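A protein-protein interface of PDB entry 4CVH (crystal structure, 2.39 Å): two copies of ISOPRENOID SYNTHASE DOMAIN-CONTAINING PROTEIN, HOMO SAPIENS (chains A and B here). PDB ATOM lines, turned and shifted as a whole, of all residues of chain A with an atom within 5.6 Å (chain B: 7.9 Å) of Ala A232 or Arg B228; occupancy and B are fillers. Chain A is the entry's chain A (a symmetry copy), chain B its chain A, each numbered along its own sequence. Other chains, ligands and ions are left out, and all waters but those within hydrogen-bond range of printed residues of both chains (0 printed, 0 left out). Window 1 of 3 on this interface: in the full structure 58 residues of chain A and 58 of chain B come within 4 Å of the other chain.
The guanidinium group (NE) of Arg B228 sits at hydrogen-bond distance from the backbone carbonyl oxygen (O) of Pro A219, at 3.0 Å.
The side-chain carboxylate (OD2) of Asp B229 is in hydrogen-bond range of the backbone NH (N) of Tyr B226 (2.9 Å).
The backbone carbonyl oxygen (O) of Tyr B231 lies within hydrogen-bond range of the side-chain hydroxyl (OG) of Ser B235 (3.3 Å).
NE1 of Trp B222 sits at hydrogen-bond distance from OD1 of Asp B229 (2.9 Å).
OD1 of Asp B229 lies within salt-bridge range of NH1 of Arg B228 (3.7 Å).
NE1 of Trp A222 sits at hydrogen-bond distance from OD1 of Asp A229, 2.9 Å away.
NH1 of Arg A228 lies within salt-bridge range of OD1 of Asp A229 (3.7 Å).
Among the printed residues, merely in contact across the chains: Pro A219 with Tyr B226, Trp A222 with Arg B228, Arg A228 with Trp B222, Arg A228 with Ala B232, Tyr A231 with Ser B235, Ala A232 with Arg B228, Ser A235 with Tyr B231 and Ile A236 with Tyr B231.
Of chain A, only Pro A219 (3.0 Å), Trp A222 (3.5 Å) and Ala A232 (3.4 Å) come within 4 Å of Arg B228.
No residue of chain B comes within 4 Å of Ala A233.
Printed residues of chain B within 4 Å of Ser A235: Tyr B231.
Printed residues of chain A within 4 Å of Ser B235: Tyr A231.
Of the printed residues of chain B, Ile A236 touches Tyr B231.
Of the printed residues of chain A, Tyr B231 touches Ser A235 (3.7 Å) and Ile A236 (3.8 Å).
The nearest residue of chain A that does not touch Arg B228 is Ile A236 (4.1 Å).
The nearest printed residue of chain A that does not touch Trp B222 is Asp A229 (6.4 Å).
Hydrophobic or aromatic side chains of chain A within 4 Å of the printed part of chain B: Pro A219, Trp A222, Tyr A231, Ala A232 and Ile A236.
Hydrophobic or aromatic side chains of chain B within 4 Å of the printed part of chain A: Trp B222, Tyr B226, Tyr B231 and Ala B232.
Among the printed residues, 9 pairs touch across the chains.
Trp A222 touches Arg B228, and with the chains exchanged Arg A228 touches Trp B222.
Arg A228 touches Ala B232, and with the chains exchanged Ala A232 touches Arg B228.
Tyr A231 touches Ser B235, and with the chains exchanged Ser A235 touches Tyr B231.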
ATOM      1  N   PHE A 121      11.697   0.620  13.627  1.00  0.00           N
ATOM      2  CA  PHE A 121      13.147   0.797  13.498  1.00  0.00           C
ATOM      3  C   PHE A 121      13.506   0.826  12.030  1.00  0.00           C
ATOM      4  O   PHE A 121      14.125  -0.091  11.480  1.00  0.00           O
ATOM      5  CB  PHE A 121      13.927  -0.297  14.241  1.00  0.00           C
ATOM      6  CG  PHE A 121      13.441  -0.521  15.626  1.00  0.00           C
ATOM      7  CD1 PHE A 121      13.521   0.494  16.563  1.00  0.00           C
ATOM      8  CD2 PHE A 121      12.858  -1.721  15.984  1.00  0.00           C
ATOM      9  CE1 PHE A 121      13.058   0.300  17.842  1.00  0.00           C
ATOM     10  CE2 PHE A 121      12.393  -1.921  17.265  1.00  0.00           C
ATOM     11  CZ  PHE A 121      12.488  -0.909  18.196  1.00  0.00           C
ATOM     12  N   PRO A 219      18.298  -6.752  10.006  1.00  0.00           N
ATOM     13  CA  PRO A 219      17.377  -7.496  10.872  1.00  0.00           C
ATOM     14  C   PRO A 219      16.377  -6.605  11.634  1.00  0.00           C
ATOM     15  O   PRO A 219      15.323  -7.094  12.044  1.00  0.00           O
ATOM     16  CB  PRO A 219      18.315  -8.210  11.862  1.00  0.00           C
ATOM     17  CG  PRO A 219      19.678  -8.159  11.253  1.00  0.00           C
ATOM     18  CD  PRO A 219      19.707  -6.922  10.412  1.00  0.00           C
ATOM     19  N   ASP A 220      16.706  -5.318  11.795  1.00  0.00           N
ATOM     20  CA  ASP A 220      15.827  -4.318  12.441  1.00  0.00           C
ATOM     21  C   ASP A 220      14.484  -4.042  11.734  1.00  0.00           C
ATOM     22  O   ASP A 220      13.575  -3.487  12.346  1.00  0.00           O
ATOM     23  CB  ASP A 220      16.556  -2.965  12.577  1.00  0.00           C
ATOM     24  CG  ASP A 220      17.848  -3.051  13.395  1.00  0.00           C
ATOM     25  OD1 ASP A 220      18.192  -4.152  13.886  1.00  0.00           O
ATOM     26  OD2 ASP A 220      18.521  -2.002  13.545  1.00  0.00           O
ATOM     27  N   TRP A 222      11.980  -5.922  10.834  1.00  0.00           N
ATOM     28  CA  TRP A 222      10.880  -6.848  11.063  1.00  0.00           C
ATOM     29  C   TRP A 222       9.608  -6.202  11.625  1.00  0.00           C
ATOM     30  O   TRP A 222       9.631  -5.129  12.253  1.00  0.00           O
ATOM     31  CB  TRP A 222      11.342  -8.014  11.943  1.00  0.00           C
ATOM     32  CG  TRP A 222      10.958  -7.960  13.404  1.00  0.00           C
ATOM     33  CD1 TRP A 222      10.064  -8.784  14.040  1.00  0.00           C
ATOM     34  CD2 TRP A 222      11.487  -7.082  14.417  1.00  0.00           C
ATOM     35  NE1 TRP A 222       9.995  -8.458  15.374  1.00  0.00           N
ATOM     36  CE2 TRP A 222      10.850  -7.416  15.630  1.00  0.00           C
ATOM     37  CE3 TRP A 222      12.425  -6.049  14.413  1.00  0.00           C
ATOM     38  CZ2 TRP A 222      11.118  -6.755  16.823  1.00  0.00           C
ATOM     39  CZ3 TRP A 222      12.680  -5.381  15.607  1.00  0.00           C
ATOM     40  CH2 TRP A 222      12.032  -5.743  16.792  1.00  0.00           C
ATOM     41  N   LYS A 227       3.480 -10.794  21.015  1.00  0.00           N
ATOM     42  CA  LYS A 227       3.930 -10.303  22.310  1.00  0.00           C
ATOM     43  C   LYS A 227       5.467 -10.329  22.371  1.00  0.00           C
ATOM     44  O   LYS A 227       6.094  -9.361  22.750  1.00  0.00           O
ATOM     45  CB  LYS A 227       3.284 -11.127  23.439  1.00  0.00           C
ATOM     46  CG  LYS A 227       3.740 -10.799  24.861  1.00  0.00           C
ATOM     47  CD  LYS A 227       3.380  -9.374  25.272  1.00  0.00           C
ATOM     48  N   ARG A 228       6.074 -11.419  21.956  1.00  0.00           N
ATOM     49  CA  ARG A 228       7.521 -11.504  21.978  1.00  0.00           C
ATOM     50  C   ARG A 228       8.229 -10.428  21.144  1.00  0.00           C
ATOM     51  O   ARG A 228       9.356 -10.055  21.479  1.00  0.00           O
ATOM     52  CB  ARG A 228       7.976 -12.878  21.526  1.00  0.00           C
ATOM     53  CG  ARG A 228       7.572 -13.273  20.124  1.00  0.00           C
ATOM     54  CD  ARG A 228       8.247 -14.584  19.783  1.00  0.00           C
ATOM     55  NE  ARG A 228       7.613 -15.268  18.665  1.00  0.00           N
ATOM     56  CZ  ARG A 228       7.872 -15.039  17.386  1.00  0.00           C
ATOM     57  NH1 ARG A 228       8.755 -14.120  17.022  1.00  0.00           N
ATOM     58  NH2 ARG A 228       7.239 -15.740  16.459  1.00  0.00           N
ATOM     59  N   ASP A 229       7.587  -9.949  20.069  1.00  0.00           N
ATOM     60  CA  ASP A 229       8.124  -8.821  19.290  1.00  0.00           C
ATOM     61  C   ASP A 229       8.032  -7.513  20.078  1.00  0.00           C
ATOM     62  O   ASP A 229       8.937  -6.679  20.004  1.00  0.00           O
ATOM     63  CB  ASP A 229       7.388  -8.639  17.959  1.00  0.00           C
ATOM     64  CG  ASP A 229       7.485  -9.848  17.061  1.00  0.00           C
ATOM     65  OD1 ASP A 229       8.593 -10.448  16.995  1.00  0.00           O
ATOM     66  OD2 ASP A 229       6.448 -10.178  16.412  1.00  0.00           O
ATOM     67  N   LEU A 230       6.940  -7.323  20.818  1.00  0.00           N
ATOM     68  CA  LEU A 230       6.841  -6.180  21.726  1.00  0.00           C
ATOM     69  C   LEU A 230       7.954  -6.182  22.758  1.00  0.00           C
ATOM     70  O   LEU A 230       8.523  -5.136  23.007  1.00  0.00           O
ATOM     71  CB  LEU A 230       5.469  -6.100  22.410  1.00  0.00           C
ATOM     72  CG  LEU A 230       4.276  -5.744  21.505  1.00  0.00           C
ATOM     73  CD1 LEU A 230       2.941  -5.966  22.226  1.00  0.00           C
ATOM     74  CD2 LEU A 230       4.392  -4.307  21.027  1.00  0.00           C
ATOM     75  N   TYR A 231       8.276  -7.341  23.340  1.00  0.00           N
ATOM     76  CA  TYR A 231       9.413  -7.444  24.276  1.00  0.00           C
ATOM     77  C   TYR A 231      10.710  -7.023  23.624  1.00  0.00           C
ATOM     78  O   TYR A 231      11.447  -6.195  24.159  1.00  0.00           O
ATOM     79  CB  TYR A 231       9.606  -8.867  24.787  1.00  0.00           C
ATOM     80  CG  TYR A 231       8.548  -9.398  25.721  1.00  0.00           C
ATOM     81  CD1 TYR A 231       7.795  -8.556  26.534  1.00  0.00           C
ATOM     82  CD2 TYR A 231       8.342 -10.766  25.835  1.00  0.00           C
ATOM     83  CE1 TYR A 231       6.841  -9.062  27.401  1.00  0.00           C
ATOM     84  CE2 TYR A 231       7.400 -11.281  26.703  1.00  0.00           C
ATOM     85  CZ  TYR A 231       6.653 -10.424  27.482  1.00  0.00           C
ATOM     86  OH  TYR A 231       5.722 -10.933  28.344  1.00  0.00           O
ATOM     87  N   ALA A 232      10.994  -7.601  22.459  1.00  0.00           N
ATOM     88  CA  ALA A 232      12.212  -7.271  21.741  1.00  0.00           C
ATOM     89  C   ALA A 232      12.297  -5.770  21.453  1.00  0.00           C
ATOM     90  O   ALA A 232      13.309  -5.153  21.711  1.00  0.00           O
ATOM     91  CB  ALA A 232      12.280  -8.060  20.465  1.00  0.00           C
ATOM     92  N   ALA A 233      11.215  -5.188  20.958  1.00  0.00           N
ATOM     93  CA  ALA A 233      11.184  -3.772  20.612  1.00  0.00           C
ATOM     94  C   ALA A 233      11.386  -2.850  21.821  1.00  0.00           C
ATOM     95  O   ALA A 233      12.085  -1.842  21.731  1.00  0.00           O
ATOM     96  CB  ALA A 233       9.875  -3.435  19.916  1.00  0.00           C
ATOM     97  N   GLU A 234      10.748  -3.179  22.935  1.00  0.00           N
ATOM     98  CA  GLU A 234      10.978  -2.474  24.180  1.00  0.00           C
ATOM     99  C   GLU A 234      12.469  -2.451  24.528  1.00  0.00           C
ATOM    100  O   GLU A 234      13.002  -1.410  24.888  1.00  0.00           O
ATOM    101  CB  GLU A 234      10.235  -3.135  25.324  1.00  0.00           C
ATOM    102  CG  GLU A 234      10.137  -2.232  26.540  1.00  0.00           C
ATOM    103  CD  GLU A 234       9.504  -2.911  27.735  1.00  0.00           C
ATOM    104  OE1 GLU A 234       9.025  -4.059  27.604  1.00  0.00           O
ATOM    105  OE2 GLU A 234       9.514  -2.303  28.823  1.00  0.00           O
ATOM    106  N   SER A 235      13.125  -3.606  24.432  1.00  0.00           N
ATOM    107  CA  SER A 235      14.537  -3.720  24.776  1.00  0.00           C
ATOM    108  C   SER A 235      15.411  -2.872  23.876  1.00  0.00           C
ATOM    109  O   SER A 235      16.343  -2.220  24.344  1.00  0.00           O
ATOM    110  CB  SER A 235      15.006  -5.166  24.689  1.00  0.00           C
ATOM    111  OG  SER A 235      14.352  -5.945  25.645  1.00  0.00           O
ATOM    112  N   ILE A 236      15.115  -2.885  22.585  1.00  0.00           N
ATOM    113  CA  ILE A 236      15.902  -2.117  21.636  1.00  0.00           C
ATOM    114  C   ILE A 236      15.715  -0.630  21.910  1.00  0.00           C
ATOM    115  O   ILE A 236      16.673   0.135  21.879  1.00  0.00           O
ATOM    116  CB  ILE A 236      15.525  -2.464  20.192  1.00  0.00           C
ATOM    117  CG1 ILE A 236      15.953  -3.893  19.885  1.00  0.00           C
ATOM    118  CG2 ILE A 236      16.197  -1.517  19.207  1.00  0.00           C
ATOM    119  CD1 ILE A 236      15.182  -4.499  18.734  1.00  0.00           C
ATOM    120  N   ILE A 237      14.484  -0.233  22.202  1.00  0.00           N
ATOM    121  CA  ILE A 237      14.200   1.154  22.536  1.00  0.00           C
ATOM    122  C   ILE A 237      14.991   1.586  23.767  1.00  0.00           C
ATOM    123  O   ILE A 237      15.667   2.596  23.723  1.00  0.00           O
ATOM    124  CB  ILE A 237      12.688   1.395  22.686  1.00  0.00           C
ATOM    125  CG1 ILE A 237      12.073   1.428  21.280  1.00  0.00           C
ATOM    126  CG2 ILE A 237      12.407   2.705  23.418  1.00  0.00           C
ATOM    127  CD1 ILE A 237      10.575   1.262  21.250  1.00  0.00           C
ATOM    128  N   LYS B  26      23.221 -19.312  17.595  1.00  0.00           N
ATOM    129  CA  LYS B  26      23.219 -18.737  18.926  1.00  0.00           C
ATOM    130  C   LYS B  26      23.090 -19.765  20.048  1.00  0.00           C
ATOM    131  O   LYS B  26      22.793 -19.401  21.172  1.00  0.00           O
ATOM    132  CB  LYS B  26      22.075 -17.737  19.024  1.00  0.00           C
ATOM    133  CG  LYS B  26      22.102 -16.667  17.951  1.00  0.00           C
ATOM    134  CD  LYS B  26      22.358 -15.311  18.572  1.00  0.00           C
ATOM    135  CE  LYS B  26      22.373 -14.200  17.549  1.00  0.00           C
ATOM    136  NZ  LYS B  26      23.426 -14.439  16.536  1.00  0.00           N
ATOM    137  N   TRP B 222       9.261 -20.180  17.643  1.00  0.00           N
ATOM    138  CA  TRP B 222      10.213 -19.547  16.740  1.00  0.00           C
ATOM    139  C   TRP B 222      11.685 -19.798  17.088  1.00  0.00           C
ATOM    140  O   TRP B 222      12.055 -20.097  18.237  1.00  0.00           O
ATOM    141  CB  TRP B 222       9.920 -18.048  16.626  1.00  0.00           C
ATOM    142  CG  TRP B 222      10.803 -17.117  17.426  1.00  0.00           C
ATOM    143  CD1 TRP B 222      11.725 -16.237  16.919  1.00  0.00           C
ATOM    144  CD2 TRP B 222      10.813 -16.932  18.855  1.00  0.00           C
ATOM    145  NE1 TRP B 222      12.314 -15.536  17.945  1.00  0.00           N
ATOM    146  CE2 TRP B 222      11.780 -15.945  19.139  1.00  0.00           C
ATOM    147  CE3 TRP B 222      10.107 -17.506  19.914  1.00  0.00           C
ATOM    148  CZ2 TRP B 222      12.061 -15.523  20.434  1.00  0.00           C
ATOM    149  CZ3 TRP B 222      10.401 -17.089  21.209  1.00  0.00           C
ATOM    150  CH2 TRP B 222      11.364 -16.105  21.452  1.00  0.00           C
ATOM    151  N   LYS B 223      12.534 -19.686  16.078  1.00  0.00           N
ATOM    152  CA  LYS B 223      13.930 -19.904  16.319  1.00  0.00           C
ATOM    153  C   LYS B 223      14.703 -18.620  16.640  1.00  0.00           C
ATOM    154  O   LYS B 223      14.525 -17.576  16.014  1.00  0.00           O
ATOM    155  CB  LYS B 223      14.557 -20.725  15.204  1.00  0.00           C
ATOM    156  CG  LYS B 223      14.967 -20.005  13.949  1.00  0.00           C
ATOM    157  CD  LYS B 223      15.625 -21.002  12.996  1.00  0.00           C
ATOM    158  CE  LYS B 223      16.950 -21.515  13.547  1.00  0.00           C
ATOM    159  NZ  LYS B 223      17.614 -22.483  12.638  1.00  0.00           N
ATOM    160  N   VAL B 224      15.546 -18.720  17.657  1.00  0.00           N
ATOM    161  CA  VAL B 224      16.391 -17.615  18.053  1.00  0.00           C
ATOM    162  C   VAL B 224      17.536 -17.493  17.051  1.00  0.00           C
ATOM    163  O   VAL B 224      18.444 -18.312  17.036  1.00  0.00           O
ATOM    164  CB  VAL B 224      16.915 -17.839  19.478  1.00  0.00           C
ATOM    165  CG1 VAL B 224      17.898 -16.755  19.873  1.00  0.00           C
ATOM    166  CG2 VAL B 224      15.744 -17.889  20.442  1.00  0.00           C
ATOM    167  N   THR B 225      17.463 -16.481  16.200  1.00  0.00           N
ATOM    168  CA  THR B 225      18.455 -16.249  15.136  1.00  0.00           C
ATOM    169  C   THR B 225      19.240 -14.937  15.313  1.00  0.00           C
ATOM    170  O   THR B 225      20.414 -14.867  14.981  1.00  0.00           O
ATOM    171  CB  THR B 225      17.761 -16.152  13.758  1.00  0.00           C
ATOM    172  OG1 THR B 225      16.865 -17.252  13.572  1.00  0.00           O
ATOM    173  CG2 THR B 225      18.792 -16.139  12.629  1.00  0.00           C
ATOM    174  N   TYR B 226      18.575 -13.890  15.790  1.00  0.00           N
ATOM    175  CA  TYR B 226      19.163 -12.557  15.848  1.00  0.00           C
ATOM    176  C   TYR B 226      19.273 -12.078  17.273  1.00  0.00           C
ATOM    177  O   TYR B 226      18.711 -12.681  18.183  1.00  0.00           O
ATOM    178  CB  TYR B 226      18.280 -11.575  15.082  1.00  0.00           C
ATOM    179  CG  TYR B 226      18.051 -11.962  13.641  1.00  0.00           C
ATOM    180  CD1 TYR B 226      19.081 -11.877  12.710  1.00  0.00           C
ATOM    181  CD2 TYR B 226      16.797 -12.387  13.201  1.00  0.00           C
ATOM    182  CE1 TYR B 226      18.876 -12.210  11.385  1.00  0.00           C
ATOM    183  CE2 TYR B 226      16.581 -12.727  11.877  1.00  0.00           C
ATOM    184  CZ  TYR B 226      17.624 -12.641  10.976  1.00  0.00           C
ATOM    185  OH  TYR B 226      17.428 -12.985   9.663  1.00  0.00           O
ATOM    186  N   LYS B 227      19.965 -10.959  17.450  1.00  0.00           N
ATOM    187  CA  LYS B 227      20.088 -10.319  18.752  1.00  0.00           C
ATOM    188  C   LYS B 227      18.690 -10.019  19.319  1.00  0.00           C
ATOM    189  O   LYS B 227      18.397 -10.327  20.456  1.00  0.00           O
ATOM    190  CB  LYS B 227      20.957  -9.053  18.636  1.00  0.00           C
ATOM    191  CG  LYS B 227      21.095  -8.210  19.904  1.00  0.00           C
ATOM    192  CD  LYS B 227      21.794  -8.965  21.031  1.00  0.00           C
ATOM    193  N   ARG B 228      17.813  -9.461  18.513  1.00  0.00           N
ATOM    194  CA  ARG B 228      16.475  -9.161  18.983  1.00  0.00           C
ATOM    195  C   ARG B 228      15.692 -10.385  19.479  1.00  0.00           C
ATOM    196  O   ARG B 228      14.831 -10.234  20.349  1.00  0.00           O
ATOM    197  CB  ARG B 228      15.681  -8.456  17.900  1.00  0.00           C
ATOM    198  CG  ARG B 228      15.492  -9.231  16.616  1.00  0.00           C
ATOM    199  CD  ARG B 228      14.546  -8.456  15.725  1.00  0.00           C
ATOM    200  NE  ARG B 228      14.625  -8.866  14.330  1.00  0.00           N
ATOM    201  CZ  ARG B 228      13.966  -9.885  13.797  1.00  0.00           C
ATOM    202  NH1 ARG B 228      13.165 -10.641  14.534  1.00  0.00           N
ATOM    203  NH2 ARG B 228      14.111 -10.149  12.507  1.00  0.00           N
ATOM    204  N   ASP B 229      15.975 -11.572  18.925  1.00  0.00           N
ATOM    205  CA  ASP B 229      15.378 -12.820  19.431  1.00  0.00           C
ATOM    206  C   ASP B 229      15.946 -13.187  20.804  1.00  0.00           C
ATOM    207  O   ASP B 229      15.215 -13.677  21.667  1.00  0.00           O
ATOM    208  CB  ASP B 229      15.610 -13.996  18.478  1.00  0.00           C
ATOM    209  CG  ASP B 229      15.013 -13.774  17.110  1.00  0.00           C
ATOM    210  OD1 ASP B 229      13.876 -13.233  17.043  1.00  0.00           O
ATOM    211  OD2 ASP B 229      15.686 -14.163  16.109  1.00  0.00           O
ATOM    212  N   LEU B 230      17.246 -12.968  21.002  1.00  0.00           N
ATOM    213  CA  LEU B 230      17.837 -13.138  22.330  1.00  0.00           C
ATOM    214  C   LEU B 230      17.179 -12.238  23.360  1.00  0.00           C
ATOM    215  O   LEU B 230      16.906 -12.700  24.451  1.00  0.00           O
ATOM    216  CB  LEU B 230      19.358 -12.925  22.318  1.00  0.00           C
ATOM    217  CG  LEU B 230      20.190 -13.994  21.587  1.00  0.00           C
ATOM    218  CD1 LEU B 230      21.642 -13.539  21.398  1.00  0.00           C
ATOM    219  CD2 LEU B 230      20.136 -15.309  22.344  1.00  0.00           C
ATOM    220  N   TYR B 231      16.910 -10.974  23.017  1.00  0.00           N
ATOM    221  CA  TYR B 231      16.181 -10.068  23.926  1.00  0.00           C
ATOM    222  C   TYR B 231      14.818 -10.617  24.283  1.00  0.00           C
ATOM    223  O   TYR B 231      14.459 -10.701  25.457  1.00  0.00           O
ATOM    224  CB  TYR B 231      15.964  -8.692  23.308  1.00  0.00           C
ATOM    225  CG  TYR B 231      17.189  -7.830  23.132  1.00  0.00           C
ATOM    226  CD1 TYR B 231      18.304  -7.959  23.956  1.00  0.00           C
ATOM    227  CD2 TYR B 231      17.207  -6.834  22.166  1.00  0.00           C
ATOM    228  CE1 TYR B 231      19.412  -7.147  23.794  1.00  0.00           C
ATOM    229  CE2 TYR B 231      18.305  -6.012  22.003  1.00  0.00           C
ATOM    230  CZ  TYR B 231      19.403  -6.175  22.818  1.00  0.00           C
ATOM    231  OH  TYR B 231      20.489  -5.359  22.658  1.00  0.00           O
ATOM    232  N   ALA B 232      14.052 -10.992  23.261  1.00  0.00           N
ATOM    233  CA  ALA B 232      12.725 -11.537  23.485  1.00  0.00           C
ATOM    234  C   ALA B 232      12.777 -12.767  24.395  1.00  0.00           C
ATOM    235  O   ALA B 232      12.033 -12.857  25.348  1.00  0.00           O
ATOM    236  CB  ALA B 232      12.085 -11.877  22.170  1.00  0.00           C
ATOM    237  N   ALA B 233      13.688 -13.687  24.113  1.00  0.00           N
ATOM    238  CA  ALA B 233      13.812 -14.918  24.886  1.00  0.00           C
ATOM    239  C   ALA B 233      14.200 -14.676  26.350  1.00  0.00           C
ATOM    240  O   ALA B 233      13.681 -15.329  27.253  1.00  0.00           O
ATOM    241  CB  ALA B 233      14.823 -15.844  24.228  1.00  0.00           C
ATOM    242  N   GLU B 234      15.135 -13.763  26.576  1.00  0.00           N
ATOM    243  CA  GLU B 234      15.476 -13.340  27.920  1.00  0.00           C
ATOM    244  C   GLU B 234      14.229 -12.880  28.681  1.00  0.00           C
ATOM    245  O   GLU B 234      14.028 -13.267  29.826  1.00  0.00           O
ATOM    246  CB  GLU B 234      16.466 -12.193  27.894  1.00  0.00           C
ATOM    247  CG  GLU B 234      17.129 -11.979  29.243  1.00  0.00           C
ATOM    248  CD  GLU B 234      18.033 -10.766  29.274  1.00  0.00           C
ATOM    249  OE1 GLU B 234      18.249 -10.136  28.215  1.00  0.00           O
ATOM    250  OE2 GLU B 234      18.506 -10.420  30.374  1.00  0.00           O
ATOM    251  N   SER B 235      13.411 -12.045  28.044  1.00  0.00           N
ATOM    252  CA  SER B 235      12.215 -11.505  28.678  1.00  0.00           C
ATOM    253  C   SER B 235      11.221 -12.590  29.033  1.00  0.00           C
ATOM    254  O   SER B 235      10.630 -12.569  30.111  1.00  0.00           O
ATOM    255  CB  SER B 235      11.528 -10.490  27.775  1.00  0.00           C
ATOM    256  OG  SER B 235      12.350  -9.379  27.582  1.00  0.00           O
